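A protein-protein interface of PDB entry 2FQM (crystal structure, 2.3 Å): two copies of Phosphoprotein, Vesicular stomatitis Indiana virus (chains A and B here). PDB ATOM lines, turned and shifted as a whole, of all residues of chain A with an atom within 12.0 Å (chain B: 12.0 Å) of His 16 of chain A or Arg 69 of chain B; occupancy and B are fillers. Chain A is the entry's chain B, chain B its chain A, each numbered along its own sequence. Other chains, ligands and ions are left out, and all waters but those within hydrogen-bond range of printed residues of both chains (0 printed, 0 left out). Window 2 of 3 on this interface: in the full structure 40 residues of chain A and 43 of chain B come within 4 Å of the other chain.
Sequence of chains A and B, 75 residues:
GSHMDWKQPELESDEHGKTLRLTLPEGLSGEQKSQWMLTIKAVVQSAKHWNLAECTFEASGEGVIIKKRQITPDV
No position is printed for both chains. Of the 12 pairs that touch across the chains among the printed residues, none has its exchanged pair printed and touching as well.
The side-chain sulfur (SG) of Cys 55 of chain B sits close to the backbone carbonyl oxygen (O) of Lys 67 of chain B, 3.7 Å away. O of Thr 56 of chain B sits at hydrogen-bond distance from N of Lys 67 of chain B (2.9 Å). The backbone carbonyl oxygen (O) of Glu 58 of chain B lies within hydrogen-bond range of the backbone NH (N) of Ile 65 of chain B (3.0 Å). The backbone carbonyl oxygen (O) of Thr 19 of chain A sits at hydrogen-bond distance from the backbone NH (N) of Glu 12 of chain A (2.6 Å).
No residue of chain B comes within 4 Å of Glu 15 of chain A. Printed residues of chain B within 4 Å of His 16 of chain A: Arg 69. Gly 17 of chain A touches two residues of chain B. Of the printed residues of chain B, Thr 19 of chain A touches Ile 65, Ile 66 and Lys 67. Of the printed residues of chain B, Leu 20 of chain A touches Ile 65 (3.4 Å) and Ile 66 (2.7 Å). Printed residues of chain A within 4 Å of Ile 66 of chain B: Thr 19 (3.5 Å) and Leu 20 (2.7 Å). Of chain A, only Gly 17 and Lys 18 come within 4 Å of Lys 68 of chain B. Arg 69 of chain B touches just these residues of chain A: His 16 (3.4 Å) and Gly 17 (3.5 Å). The nearest residue of chain B that does not touch His 16 of chain A is Lys 68 of chain B (4.8 Å).
Leu 11 of chain A touches Trp 50 of chain B. CA of Gly 17 of chain A touches O of Lys 68 of chain B (3.5 Å). Gly 17 of chain A touches Arg 69 of chain B. CB of Lys 18 of chain A touches CZ2 of Trp 50 of chain B, 3.96 Å away. Lys 67 of chain B touches Lys 18 of chain A. Thr 19 of chain A touches Ile 65 of chain B. Thr 19 of chain A touches Ile 66 of chain B. O of Leu 20 of chain A touches CA of Ile 65 of chain B (3.4 Å).
Printed residues of chain A that touch a printed residue of chain B: Leu 11, His 16, Gly 17, Lys 18, Thr 19 and Leu 20. Hydrophobic or aromatic side chains of chain A that line the printed part of chain B: Leu 11 and Leu 20. Hydrophobic or aromatic side chains of chain B that line the printed part of chain A: Trp 50 and Ile 65. Among the printed residues, 12 pairs touch across the chains. Among the printed residues, no Asp or Glu carboxylate lies within 4 Å of a Lys or Arg side-chain nitrogen of the other chain.
N of Leu 20 of chain A sits at hydrogen-bond distance from O of Ile 66 of chain B (2.7 Å). The side-chain amino group (NZ) of Lys 67 of chain B lies within hydrogen-bond range of the side-chain hydroxyl (OG1) of Thr 19 of chain A, 3.1 Å away. O of Lys 68 of chain B lies within hydrogen-bond range of N of Lys 18 of chain A, 3.0 Å away. The backbone carbonyl oxygen (O) of His 16 of chain A sits close to the backbone carbonyl oxygen (O) of Arg 69 of chain B (3.4 Å).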
ATOM      1  N   LEU A  11     -25.862  -0.444  12.423  1.00  0.00           N
ATOM      2  CA  LEU A  11     -26.169  -0.425  11.024  1.00  0.00           C
ATOM      3  C   LEU A  11     -26.522   1.025  10.641  1.00  0.00           C
ATOM      4  O   LEU A  11     -27.551   1.581  11.088  1.00  0.00           O
ATOM      5  CB  LEU A  11     -27.339  -1.365  10.808  1.00  0.00           C
ATOM      6  CG  LEU A  11     -27.943  -1.331   9.415  1.00  0.00           C
ATOM      7  CD1 LEU A  11     -27.262  -2.364   8.497  1.00  0.00           C
ATOM      8  CD2 LEU A  11     -29.418  -1.581   9.561  1.00  0.00           C
ATOM      9  N   GLU A  12     -25.654   1.667   9.861  1.00  0.00           N
ATOM     10  CA  GLU A  12     -25.927   3.046   9.442  1.00  0.00           C
ATOM     11  C   GLU A  12     -26.576   2.981   8.056  1.00  0.00           C
ATOM     12  O   GLU A  12     -26.141   2.292   7.146  1.00  0.00           O
ATOM     13  CB  GLU A  12     -24.631   3.870   9.373  1.00  0.00           C
ATOM     14  CG  GLU A  12     -23.729   3.798  10.664  1.00  0.00           C
ATOM     15  CD  GLU A  12     -22.253   4.258  10.471  1.00  0.00           C
ATOM     16  OE1 GLU A  12     -21.369   3.843  11.282  1.00  0.00           O
ATOM     17  OE2 GLU A  12     -21.976   5.027   9.526  1.00  0.00           O
ATOM     18  N   SER A  13     -27.648   3.702   7.911  1.00  0.00           N
ATOM     19  CA  SER A  13     -28.327   3.720   6.652  1.00  0.00           C
ATOM     20  C   SER A  13     -28.084   5.107   6.040  1.00  0.00           C
ATOM     21  O   SER A  13     -28.438   6.136   6.635  1.00  0.00           O
ATOM     22  CB  SER A  13     -29.808   3.475   6.898  1.00  0.00           C
ATOM     23  OG  SER A  13     -30.533   3.527   5.705  1.00  0.00           O
ATOM     24  N   ASP A  14     -27.430   5.104   4.880  1.00  0.00           N
ATOM     25  CA  ASP A  14     -27.102   6.307   4.102  1.00  0.00           C
ATOM     26  C   ASP A  14     -28.046   6.309   2.909  1.00  0.00           C
ATOM     27  O   ASP A  14     -28.619   5.277   2.546  1.00  0.00           O
ATOM     28  CB  ASP A  14     -25.679   6.233   3.516  1.00  0.00           C
ATOM     29  CG  ASP A  14     -24.603   6.590   4.503  1.00  0.00           C
ATOM     30  OD1 ASP A  14     -24.274   7.789   4.584  1.00  0.00           O
ATOM     31  OD2 ASP A  14     -24.084   5.679   5.189  1.00  0.00           O
ATOM     32  N   GLU A  15     -28.176   7.468   2.283  1.00  0.00           N
ATOM     33  CA  GLU A  15     -29.011   7.610   1.099  1.00  0.00           C
ATOM     34  C   GLU A  15     -28.210   6.885  -0.001  1.00  0.00           C
ATOM     35  O   GLU A  15     -28.751   6.500  -1.039  1.00  0.00           O
ATOM     36  CB  GLU A  15     -29.162   9.102   0.773  1.00  0.00           C
ATOM     37  CG  GLU A  15     -30.138   9.452  -0.365  1.00  0.00           C
ATOM     38  CD  GLU A  15     -30.134  10.966  -0.718  1.00  0.00           C
ATOM     39  OE1 GLU A  15     -29.102  11.457  -1.245  1.00  0.00           O
ATOM     40  OE2 GLU A  15     -31.151  11.668  -0.468  1.00  0.00           O
ATOM     41  N   HIS A  16     -26.918   6.684   0.274  1.00  0.00           N
ATOM     42  CA  HIS A  16     -25.992   6.038  -0.643  1.00  0.00           C
ATOM     43  C   HIS A  16     -25.710   4.551  -0.329  1.00  0.00           C
ATOM     44  O   HIS A  16     -24.827   3.935  -0.911  1.00  0.00           O
ATOM     45  CB  HIS A  16     -24.700   6.854  -0.666  1.00  0.00           C
ATOM     46  CG  HIS A  16     -24.934   8.339  -0.704  1.00  0.00           C
ATOM     47  ND1 HIS A  16     -25.183   9.033  -1.871  1.00  0.00           N
ATOM     48  CD2 HIS A  16     -25.033   9.249   0.299  1.00  0.00           C
ATOM     49  CE1 HIS A  16     -25.425  10.303  -1.587  1.00  0.00           C
ATOM     50  NE2 HIS A  16     -25.342  10.460  -0.277  1.00  0.00           N
ATOM     51  N   GLY A  17     -26.473   3.971   0.584  1.00  0.00           N
ATOM     52  CA  GLY A  17     -26.280   2.573   0.916  1.00  0.00           C
ATOM     53  C   GLY A  17     -26.271   2.360   2.408  1.00  0.00           C
ATOM     54  O   GLY A  17     -26.502   3.286   3.156  1.00  0.00           O
ATOM     55  N   LYS A  18     -26.007   1.138   2.846  1.00  0.00           N
ATOM     56  CA  LYS A  18     -25.957   0.823   4.280  1.00  0.00           C
ATOM     57  C   LYS A  18     -24.570   0.461   4.749  1.00  0.00           C
ATOM     58  O   LYS A  18     -23.703   0.082   3.973  1.00  0.00           O
ATOM     59  CB  LYS A  18     -26.914  -0.330   4.636  1.00  0.00           C
ATOM     60  CG  LYS A  18     -28.366   0.039   4.404  1.00  0.00           C
ATOM     61  CD  LYS A  18     -29.262  -1.061   4.863  1.00  0.00           C
ATOM     62  CE  LYS A  18     -30.676  -0.608   4.725  1.00  0.00           C
ATOM     63  NZ  LYS A  18     -30.940  -0.307   3.305  1.00  0.00           N
ATOM     64  N   THR A  19     -24.371   0.560   6.041  1.00  0.00           N
ATOM     65  CA  THR A  19     -23.068   0.246   6.607  1.00  0.00           C
ATOM     66  C   THR A  19     -23.185  -0.464   7.954  1.00  0.00           C
ATOM     67  O   THR A  19     -23.795   0.074   8.889  1.00  0.00           O
ATOM     68  CB  THR A  19     -22.253   1.534   6.778  1.00  0.00           C
ATOM     69  OG1 THR A  19     -22.237   2.257   5.531  1.00  0.00           O
ATOM     70  CG2 THR A  19     -20.836   1.220   7.189  1.00  0.00           C
ATOM     71  N   LEU A  20     -22.642  -1.686   8.034  1.00  0.00           N
ATOM     72  CA  LEU A  20     -22.628  -2.447   9.292  1.00  0.00           C
ATOM     73  C   LEU A  20     -21.309  -2.137  10.014  1.00  0.00           C
ATOM     74  O   LEU A  20     -20.239  -2.378   9.501  1.00  0.00           O
ATOM     75  CB  LEU A  20     -22.791  -3.954   9.064  1.00  0.00           C
ATOM     76  CG  LEU A  20     -22.623  -4.795  10.351  1.00  0.00           C
ATOM     77  CD1 LEU A  20     -23.917  -4.782  11.187  1.00  0.00           C
ATOM     78  CD2 LEU A  20     -22.323  -6.191  10.002  1.00  0.00           C
ATOM     79  N   HIS B  49     -28.494 -11.903   5.076  1.00  0.00           N
ATOM     80  CA  HIS B  49     -29.381 -10.927   4.429  1.00  0.00           C
ATOM     81  C   HIS B  49     -28.761 -10.314   3.178  1.00  0.00           C
ATOM     82  O   HIS B  49     -29.476  -9.971   2.235  1.00  0.00           O
ATOM     83  CB  HIS B  49     -29.715  -9.755   5.373  1.00  0.00           C
ATOM     84  CG  HIS B  49     -30.622 -10.110   6.505  1.00  0.00           C
ATOM     85  ND1 HIS B  49     -30.177 -10.689   7.674  1.00  0.00           N
ATOM     86  CD2 HIS B  49     -31.959  -9.959   6.650  1.00  0.00           C
ATOM     87  CE1 HIS B  49     -31.198 -10.881   8.489  1.00  0.00           C
ATOM     88  NE2 HIS B  49     -32.291 -10.444   7.892  1.00  0.00           N
ATOM     89  N   TRP B  50     -27.440 -10.136   3.221  1.00  0.00           N
ATOM     90  CA  TRP B  50     -26.639  -9.537   2.153  1.00  0.00           C
ATOM     91  C   TRP B  50     -25.699 -10.578   1.567  1.00  0.00           C
ATOM     92  O   TRP B  50     -25.441 -11.593   2.182  1.00  0.00           O
ATOM     93  CB  TRP B  50     -25.715  -8.427   2.690  1.00  0.00           C
ATOM     94  CG  TRP B  50     -26.378  -7.289   3.385  1.00  0.00           C
ATOM     95  CD1 TRP B  50     -27.704  -6.941   3.322  1.00  0.00           C
ATOM     96  CD2 TRP B  50     -25.739  -6.276   4.175  1.00  0.00           C
ATOM     97  NE1 TRP B  50     -27.924  -5.782   4.010  1.00  0.00           N
ATOM     98  CE2 TRP B  50     -26.738  -5.344   4.539  1.00  0.00           C
ATOM     99  CE3 TRP B  50     -24.419  -6.054   4.594  1.00  0.00           C
ATOM    100  CZ2 TRP B  50     -26.459  -4.206   5.293  1.00  0.00           C
ATOM    101  CZ3 TRP B  50     -24.131  -4.917   5.339  1.00  0.00           C
ATOM    102  CH2 TRP B  50     -25.156  -4.000   5.683  1.00  0.00           C
ATOM    103  N   ASN B  51     -25.173 -10.313   0.384  1.00  0.00           N
ATOM    104  CA  ASN B  51     -24.206 -11.215  -0.222  1.00  0.00           C
ATOM    105  C   ASN B  51     -22.928 -10.478   0.026  1.00  0.00           C
ATOM    106  O   ASN B  51     -22.636  -9.463  -0.651  1.00  0.00           O
ATOM    107  CB  ASN B  51     -24.421 -11.389  -1.719  1.00  0.00           C
ATOM    108  CG  ASN B  51     -23.452 -12.396  -2.326  1.00  0.00           C
ATOM    109  OD1 ASN B  51     -23.790 -13.139  -3.250  1.00  0.00           O
ATOM    110  ND2 ASN B  51     -22.239 -12.411  -1.821  1.00  0.00           N
ATOM    111  N   LEU B  52     -22.153 -10.996   0.978  1.00  0.00           N
ATOM    112  CA  LEU B  52     -20.932 -10.331   1.390  1.00  0.00           C
ATOM    113  C   LEU B  52     -19.855 -10.258   0.303  1.00  0.00           C
ATOM    114  O   LEU B  52     -18.919  -9.487   0.465  1.00  0.00           O
ATOM    115  CB  LEU B  52     -20.359 -10.958   2.661  1.00  0.00           C
ATOM    116  CG  LEU B  52     -21.238 -10.958   3.927  1.00  0.00           C
ATOM    117  CD1 LEU B  52     -20.423 -11.339   5.174  1.00  0.00           C
ATOM    118  CD2 LEU B  52     -21.849  -9.552   4.099  1.00  0.00           C
ATOM    119  N   ALA B  53     -19.992 -11.022  -0.790  1.00  0.00           N
ATOM    120  CA  ALA B  53     -19.019 -10.974  -1.888  1.00  0.00           C
ATOM    121  C   ALA B  53     -19.237  -9.705  -2.670  1.00  0.00           C
ATOM    122  O   ALA B  53     -18.421  -9.330  -3.517  1.00  0.00           O
ATOM    123  CB  ALA B  53     -19.202 -12.149  -2.838  1.00  0.00           C
ATOM    124  N   GLU B  54     -20.369  -9.059  -2.414  1.00  0.00           N
ATOM    125  CA  GLU B  54     -20.685  -7.837  -3.105  1.00  0.00           C
ATOM    126  C   GLU B  54     -20.679  -6.705  -2.116  1.00  0.00           C
ATOM    127  O   GLU B  54     -21.277  -5.675  -2.386  1.00  0.00           O
ATOM    128  CB  GLU B  54     -22.046  -7.964  -3.794  1.00  0.00           C
ATOM    129  CG  GLU B  54     -22.075  -9.052  -4.794  1.00  0.00           C
ATOM    130  CD  GLU B  54     -21.279  -8.673  -6.016  1.00  0.00           C
ATOM    131  OE1 GLU B  54     -21.390  -9.356  -7.040  1.00  0.00           O
ATOM    132  OE2 GLU B  54     -20.536  -7.677  -5.962  1.00  0.00           O
ATOM    133  N   CYS B  55     -19.993  -6.885  -0.982  1.00  0.00           N
ATOM    134  CA  CYS B  55     -19.912  -5.818   0.033  1.00  0.00           C
ATOM    135  C   CYS B  55     -18.474  -5.449   0.232  1.00  0.00           C
ATOM    136  O   CYS B  55     -17.599  -6.250  -0.038  1.00  0.00           O
ATOM    137  CB  CYS B  55     -20.502  -6.257   1.404  1.00  0.00           C
ATOM    138  SG  CYS B  55     -22.308  -6.368   1.346  1.00  0.00           S
ATOM    139  N   THR B  56     -18.226  -4.256   0.735  1.00  0.00           N
ATOM    140  CA  THR B  56     -16.866  -3.856   0.983  1.00  0.00           C
ATOM    141  C   THR B  56     -16.569  -4.091   2.472  1.00  0.00           C
ATOM    142  O   THR B  56     -17.399  -3.830   3.326  1.00  0.00           O
ATOM    143  CB  THR B  56     -16.667  -2.362   0.623  1.00  0.00           C
ATOM    144  OG1 THR B  56     -16.752  -2.193  -0.795  1.00  0.00           O
ATOM    145  CG2 THR B  56     -15.328  -1.892   1.077  1.00  0.00           C
ATOM    146  N   PHE B  57     -15.392  -4.620   2.762  1.00  0.00           N
ATOM    147  CA  PHE B  57     -14.924  -4.894   4.101  1.00  0.00           C
ATOM    148  C   PHE B  57     -13.621  -4.110   4.333  1.00  0.00           C
ATOM    149  O   PHE B  57     -12.739  -4.121   3.477  1.00  0.00           O
ATOM    150  CB  PHE B  57     -14.692  -6.396   4.228  1.00  0.00           C
ATOM    151  CG  PHE B  57     -13.933  -6.808   5.463  1.00  0.00           C
ATOM    152  CD1 PHE B  57     -12.554  -6.926   5.437  1.00  0.00           C
ATOM    153  CD2 PHE B  57     -14.588  -7.027   6.671  1.00  0.00           C
ATOM    154  CE1 PHE B  57     -11.823  -7.249   6.607  1.00  0.00           C
ATOM    155  CE2 PHE B  57     -13.856  -7.354   7.860  1.00  0.00           C
ATOM    156  CZ  PHE B  57     -12.480  -7.461   7.809  1.00  0.00           C
ATOM    157  N   GLU B  58     -13.500  -3.425   5.476  1.00  0.00           N
ATOM    158  CA  GLU B  58     -12.298  -2.642   5.792  1.00  0.00           C
ATOM    159  C   GLU B  58     -12.176  -2.318   7.267  1.00  0.00           C
ATOM    160  O   GLU B  58     -13.168  -2.350   7.993  1.00  0.00           O
ATOM    161  CB  GLU B  58     -12.300  -1.330   4.990  1.00  0.00           C
ATOM    162  CG  GLU B  58     -13.275  -0.272   5.423  1.00  0.00           C
ATOM    163  CD  GLU B  58     -13.723   0.580   4.241  1.00  0.00           C
ATOM    164  OE1 GLU B  58     -13.001   0.593   3.222  1.00  0.00           O
ATOM    165  OE2 GLU B  58     -14.788   1.229   4.322  1.00  0.00           O
ATOM    166  N   ILE B  65     -15.819  -2.340   9.431  1.00  0.00           N
ATOM    167  CA  ILE B  65     -16.946  -1.898   8.617  1.00  0.00           C
ATOM    168  C   ILE B  65     -17.327  -2.874   7.444  1.00  0.00           C
ATOM    169  O   ILE B  65     -16.475  -3.514   6.844  1.00  0.00           O
ATOM    170  CB  ILE B  65     -16.561  -0.517   7.977  1.00  0.00           C
ATOM    171  CG1 ILE B  65     -16.501   0.519   9.045  1.00  0.00           C
ATOM    172  CG2 ILE B  65     -17.607  -0.003   7.052  1.00  0.00           C
ATOM    173  CD1 ILE B  65     -17.831   0.681   9.597  1.00  0.00           C
ATOM    174  N   ILE B  66     -18.602  -2.933   7.082  1.00  0.00           N
ATOM    175  CA  ILE B  66     -19.041  -3.752   5.984  1.00  0.00           C
ATOM    176  C   ILE B  66     -20.096  -2.913   5.321  1.00  0.00           C
ATOM    177  O   ILE B  66     -21.090  -2.565   5.962  1.00  0.00           O
ATOM    178  CB  ILE B  66     -19.611  -5.078   6.486  1.00  0.00           C
ATOM    179  CG1 ILE B  66     -18.492  -5.936   7.019  1.00  0.00           C
ATOM    180  CG2 ILE B  66     -20.290  -5.883   5.352  1.00  0.00           C
ATOM    181  CD1 ILE B  66     -19.010  -7.365   7.323  1.00  0.00           C
ATOM    182  N   LYS B  67     -19.858  -2.535   4.065  1.00  0.00           N
ATOM    183  CA  LYS B  67     -20.791  -1.650   3.344  1.00  0.00           C
ATOM    184  C   LYS B  67     -21.402  -2.295   2.162  1.00  0.00           C
ATOM    185  O   LYS B  67     -20.744  -3.060   1.471  1.00  0.00           O
ATOM    186  CB  LYS B  67     -20.103  -0.389   2.838  1.00  0.00           C
ATOM    187  CG  LYS B  67     -19.059   0.191   3.801  1.00  0.00           C
ATOM    188  CD  LYS B  67     -18.242   1.361   3.194  1.00  0.00           C
ATOM    189  CE  LYS B  67     -19.017   2.679   3.232  1.00  0.00           C
ATOM    190  NZ  LYS B  67     -19.426   3.119   4.618  1.00  0.00           N
ATOM    191  N   LYS B  68     -22.659  -1.968   1.936  1.00  0.00           N
ATOM    192  CA  LYS B  68     -23.457  -2.467   0.831  1.00  0.00           C
ATOM    193  C   LYS B  68     -24.045  -1.232   0.134  1.00  0.00           C
ATOM    194  O   LYS B  68     -25.029  -0.667   0.602  1.00  0.00           O
ATOM    195  CB  LYS B  68     -24.598  -3.331   1.379  1.00  0.00           C
ATOM    196  CG  LYS B  68     -25.697  -3.630   0.350  1.00  0.00           C
ATOM    197  CD  LYS B  68     -26.824  -4.458   0.900  1.00  0.00           C
ATOM    198  CE  LYS B  68     -27.998  -4.347  -0.016  1.00  0.00           C
ATOM    199  NZ  LYS B  68     -28.794  -5.619  -0.100  1.00  0.00           N
ATOM    200  N   ARG B  69     -23.461  -0.784  -0.965  1.00  0.00           N
ATOM    201  CA  ARG B  69     -24.028   0.384  -1.629  1.00  0.00           C
ATOM    202  C   ARG B  69     -25.450   0.138  -2.187  1.00  0.00           C
ATOM    203  O   ARG B  69     -26.224   1.122  -2.321  1.00  0.00           O
ATOM    204  CB  ARG B  69     -23.083   0.869  -2.724  1.00  0.00           C
ATOM    205  CG  ARG B  69     -22.797  -0.154  -3.788  1.00  0.00           C
ATOM    206  CD  ARG B  69     -22.152   0.526  -4.963  1.00  0.00           C
ATOM    207  NE  ARG B  69     -22.802   1.808  -5.240  1.00  0.00           N
ATOM    208  CZ  ARG B  69     -22.336   2.698  -6.112  1.00  0.00           C
ATOM    209  NH1 ARG B  69     -21.218   2.436  -6.792  1.00  0.00           N
ATOM    210  NH2 ARG B  69     -22.970   3.853  -6.290  1.00  0.00           N
